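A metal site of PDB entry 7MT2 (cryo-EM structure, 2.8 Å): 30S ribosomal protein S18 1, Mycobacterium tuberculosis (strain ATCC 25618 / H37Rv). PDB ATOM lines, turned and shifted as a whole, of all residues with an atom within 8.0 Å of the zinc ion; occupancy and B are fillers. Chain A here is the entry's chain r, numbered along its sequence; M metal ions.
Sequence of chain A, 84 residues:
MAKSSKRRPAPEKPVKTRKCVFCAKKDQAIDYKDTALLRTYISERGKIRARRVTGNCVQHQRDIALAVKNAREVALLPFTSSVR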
ATOM      1  N   LYS A  19     -26.504  -6.295  23.762  1.00  0.00           N
ATOM      2  CA  LYS A  19     -25.168  -6.839  23.921  1.00  0.00           C
ATOM      3  C   LYS A  19     -24.499  -6.073  25.065  1.00  0.00           C
ATOM      4  O   LYS A  19     -23.538  -6.533  25.657  1.00  0.00           O
ATOM      5  CB  LYS A  19     -24.373  -6.724  22.615  1.00  0.00           C
ATOM      6  CG  LYS A  19     -23.128  -7.593  22.510  1.00  0.00           C
ATOM      7  CD  LYS A  19     -21.863  -6.841  22.848  1.00  0.00           C
ATOM      8  CE  LYS A  19     -20.627  -7.672  22.540  1.00  0.00           C
ATOM      9  NZ  LYS A  19     -20.567  -8.880  23.411  1.00  0.00           N
ATOM     10  N   CYS A  20     -25.047  -4.899  25.361  1.00  0.00           N
ATOM     11  CA  CYS A  20     -24.623  -4.141  26.529  1.00  0.00           C
ATOM     12  C   CYS A  20     -25.156  -4.796  27.798  1.00  0.00           C
ATOM     13  O   CYS A  20     -26.300  -5.265  27.836  1.00  0.00           O
ATOM     14  CB  CYS A  20     -25.109  -2.697  26.423  1.00  0.00           C
ATOM     15  SG  CYS A  20     -24.642  -1.627  27.798  1.00  0.00           S
ATOM     16  N   VAL A  21     -24.330  -4.831  28.831  1.00  0.00           N
ATOM     17  CA  VAL A  21     -24.726  -5.474  30.082  1.00  0.00           C
ATOM     18  C   VAL A  21     -25.736  -4.603  30.829  1.00  0.00           C
ATOM     19  O   VAL A  21     -26.754  -5.098  31.326  1.00  0.00           O
ATOM     20  CB  VAL A  21     -23.492  -5.784  30.935  1.00  0.00           C
ATOM     21  CG1 VAL A  21     -23.900  -6.341  32.289  1.00  0.00           C
ATOM     22  CG2 VAL A  21     -22.601  -6.772  30.211  1.00  0.00           C
ATOM     23  N   PHE A  22     -25.480  -3.301  30.891  1.00  0.00           N
ATOM     24  CA  PHE A  22     -26.310  -2.406  31.699  1.00  0.00           C
ATOM     25  C   PHE A  22     -27.672  -2.146  31.067  1.00  0.00           C
ATOM     26  O   PHE A  22     -28.599  -1.771  31.782  1.00  0.00           O
ATOM     27  CB  PHE A  22     -25.591  -1.083  31.915  1.00  0.00           C
ATOM     28  CG  PHE A  22     -24.274  -1.222  32.582  1.00  0.00           C
ATOM     29  CD1 PHE A  22     -24.186  -1.453  33.939  1.00  0.00           C
ATOM     30  CD2 PHE A  22     -23.104  -1.122  31.849  1.00  0.00           C
ATOM     31  CE1 PHE A  22     -22.954  -1.600  34.542  1.00  0.00           C
ATOM     32  CE2 PHE A  22     -21.881  -1.263  32.454  1.00  0.00           C
ATOM     33  CZ  PHE A  22     -21.811  -1.500  33.797  1.00  0.00           C
ATOM     34  N   CYS A  23     -27.799  -2.331  29.756  1.00  0.00           N
ATOM     35  CA  CYS A  23     -29.100  -2.143  29.120  1.00  0.00           C
ATOM     36  C   CYS A  23     -29.972  -3.382  29.249  1.00  0.00           C
ATOM     37  O   CYS A  23     -31.198  -3.258  29.361  1.00  0.00           O
ATOM     38  CB  CYS A  23     -28.938  -1.764  27.659  1.00  0.00           C
ATOM     39  SG  CYS A  23     -28.182  -0.157  27.353  1.00  0.00           S
ATOM     40  N   ALA A  24     -29.371  -4.574  29.224  1.00  0.00           N
ATOM     41  CA  ALA A  24     -30.154  -5.798  29.372  1.00  0.00           C
ATOM     42  C   ALA A  24     -30.584  -5.995  30.813  1.00  0.00           C
ATOM     43  O   ALA A  24     -31.778  -6.035  31.112  1.00  0.00           O
ATOM     44  CB  ALA A  24     -29.339  -6.997  28.867  1.00  0.00           C
ATOM     45  N   ILE A  30     -24.396   2.406  38.250  1.00  0.00           N
ATOM     46  CA  ILE A  30     -22.953   2.473  38.115  1.00  0.00           C
ATOM     47  C   ILE A  30     -22.450   3.531  39.086  1.00  0.00           C
ATOM     48  O   ILE A  30     -22.627   4.729  38.864  1.00  0.00           O
ATOM     49  CB  ILE A  30     -22.533   2.785  36.677  1.00  0.00           C
ATOM     50  CG1 ILE A  30     -23.111   1.753  35.731  1.00  0.00           C
ATOM     51  CG2 ILE A  30     -21.030   2.780  36.572  1.00  0.00           C
ATOM     52  CD1 ILE A  30     -22.991   2.137  34.284  1.00  0.00           C
ATOM     53  N   GLY A  55     -18.687  -3.755  24.484  1.00  0.00           N
ATOM     54  CA  GLY A  55     -20.047  -3.805  24.011  1.00  0.00           C
ATOM     55  C   GLY A  55     -20.995  -2.804  24.637  1.00  0.00           C
ATOM     56  O   GLY A  55     -22.207  -2.951  24.473  1.00  0.00           O
ATOM     57  N   ASN A  56     -20.484  -1.807  25.344  1.00  0.00           N
ATOM     58  CA  ASN A  56     -21.331  -0.810  25.988  1.00  0.00           C
ATOM     59  C   ASN A  56     -21.979   0.099  24.950  1.00  0.00           C
ATOM     60  O   ASN A  56     -21.586   0.139  23.784  1.00  0.00           O
ATOM     61  CB  ASN A  56     -20.525   0.031  26.969  1.00  0.00           C
ATOM     62  CG  ASN A  56     -20.116  -0.744  28.194  1.00  0.00           C
ATOM     63  OD1 ASN A  56     -20.886  -1.535  28.730  1.00  0.00           O
ATOM     64  ND2 ASN A  56     -18.897  -0.510  28.655  1.00  0.00           N
ATOM     65  N   CYS A  57     -22.997   0.832  25.384  1.00  0.00           N
ATOM     66  CA  CYS A  57     -23.622   1.837  24.552  1.00  0.00           C
ATOM     67  C   CYS A  57     -22.919   3.171  24.772  1.00  0.00           C
ATOM     68  O   CYS A  57     -21.897   3.251  25.457  1.00  0.00           O
ATOM     69  CB  CYS A  57     -25.114   1.906  24.849  1.00  0.00           C
ATOM     70  SG  CYS A  57     -25.513   2.449  26.511  1.00  0.00           S
ATOM     71  N   VAL A  58     -23.451   4.246  24.188  1.00  0.00           N
ATOM     72  CA  VAL A  58     -22.833   5.559  24.376  1.00  0.00           C
ATOM     73  C   VAL A  58     -23.147   6.088  25.765  1.00  0.00           C
ATOM     74  O   VAL A  58     -22.291   6.695  26.422  1.00  0.00           O
ATOM     75  CB  VAL A  58     -23.301   6.525  23.280  1.00  0.00           C
ATOM     76  CG1 VAL A  58     -22.682   7.903  23.451  1.00  0.00           C
ATOM     77  CG2 VAL A  58     -22.943   5.986  21.941  1.00  0.00           C
ATOM     78  N   GLN A  59     -24.362   5.836  26.264  1.00  0.00           N
ATOM     79  CA  GLN A  59     -24.802   6.441  27.508  1.00  0.00           C
ATOM     80  C   GLN A  59     -24.112   5.822  28.713  1.00  0.00           C
ATOM     81  O   GLN A  59     -23.797   6.520  29.680  1.00  0.00           O
ATOM     82  CB  GLN A  59     -26.310   6.328  27.648  1.00  0.00           C
ATOM     83  CG  GLN A  59     -27.069   7.159  26.658  1.00  0.00           C
ATOM     84  CD  GLN A  59     -28.558   6.993  26.776  1.00  0.00           C
ATOM     85  OE1 GLN A  59     -29.037   6.220  27.601  1.00  0.00           O
ATOM     86  NE2 GLN A  59     -29.300   7.678  25.923  1.00  0.00           N
ATOM     87  N   HIS A  60     -23.866   4.520  28.687  1.00  0.00           N
ATOM     88  CA  HIS A  60     -23.251   3.868  29.837  1.00  0.00           C
ATOM     89  C   HIS A  60     -21.737   3.889  29.800  1.00  0.00           C
ATOM     90  O   HIS A  60     -21.117   3.811  30.857  1.00  0.00           O
ATOM     91  CB  HIS A  60     -23.749   2.430  29.971  1.00  0.00           C
ATOM     92  CG  HIS A  60     -25.210   2.332  30.285  1.00  0.00           C
ATOM     93  ND1 HIS A  60     -26.161   2.126  29.321  1.00  0.00           N
ATOM     94  CD2 HIS A  60     -25.867   2.432  31.456  1.00  0.00           C
ATOM     95  CE1 HIS A  60     -27.350   2.092  29.884  1.00  0.00           C
ATOM     96  NE2 HIS A  60     -27.205   2.274  31.178  1.00  0.00           N
ATOM     97  N   GLN A  61     -21.125   3.989  28.614  1.00  0.00           N
ATOM     98  CA  GLN A  61     -19.690   4.209  28.531  1.00  0.00           C
ATOM     99  C   GLN A  61     -19.294   5.540  29.148  1.00  0.00           C
ATOM    100  O   GLN A  61     -18.250   5.654  29.790  1.00  0.00           O
ATOM    101  CB  GLN A  61     -19.231   4.158  27.074  1.00  0.00           C
ATOM    102  CG  GLN A  61     -17.753   4.305  26.834  1.00  0.00           C
ATOM    103  CD  GLN A  61     -16.991   3.094  27.286  1.00  0.00           C
ATOM    104  OE1 GLN A  61     -17.438   1.970  27.135  1.00  0.00           O
ATOM    105  NE2 GLN A  61     -15.800   3.323  27.833  1.00  0.00           N
ATOM    106  N   ASP A  63     -21.054   6.737  31.597  1.00  0.00           N
ATOM    107  CA  ASP A  63     -21.247   6.481  33.013  1.00  0.00           C
ATOM    108  C   ASP A  63     -20.142   5.619  33.607  1.00  0.00           C
ATOM    109  O   ASP A  63     -19.878   5.726  34.803  1.00  0.00           O
ATOM    110  CB  ASP A  63     -22.608   5.832  33.264  1.00  0.00           C
ATOM    111  CG  ASP A  63     -23.762   6.821  33.154  1.00  0.00           C
ATOM    112  OD1 ASP A  63     -23.543   8.015  33.421  1.00  0.00           O
ATOM    113  OD2 ASP A  63     -24.885   6.402  32.806  1.00  0.00           O
HETATM  114 ZN    ZN M   1     -25.900   0.506  27.926  1.00  0.00          ZN
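The side-chain sulfur (SG) of Cys 57 sits close to the backbone NH (N) of Gln 59.
SG of Cys 20 lies close to N of Phe 22 (3.6 Å).
Four residues have an atom within 4 Å of the zinc ion: Cys 20, Cys 23, Cys 57 and His 60.
ND1 of His 60 is bound to the zinc ion.
SG of Cys 57 is bound to the zinc ion (2.4 Å).
SG of Cys 23 binds the zinc ion, at 2.4 Å.
The zinc ion is bound by SG of Cys 20 (2.5 Å).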
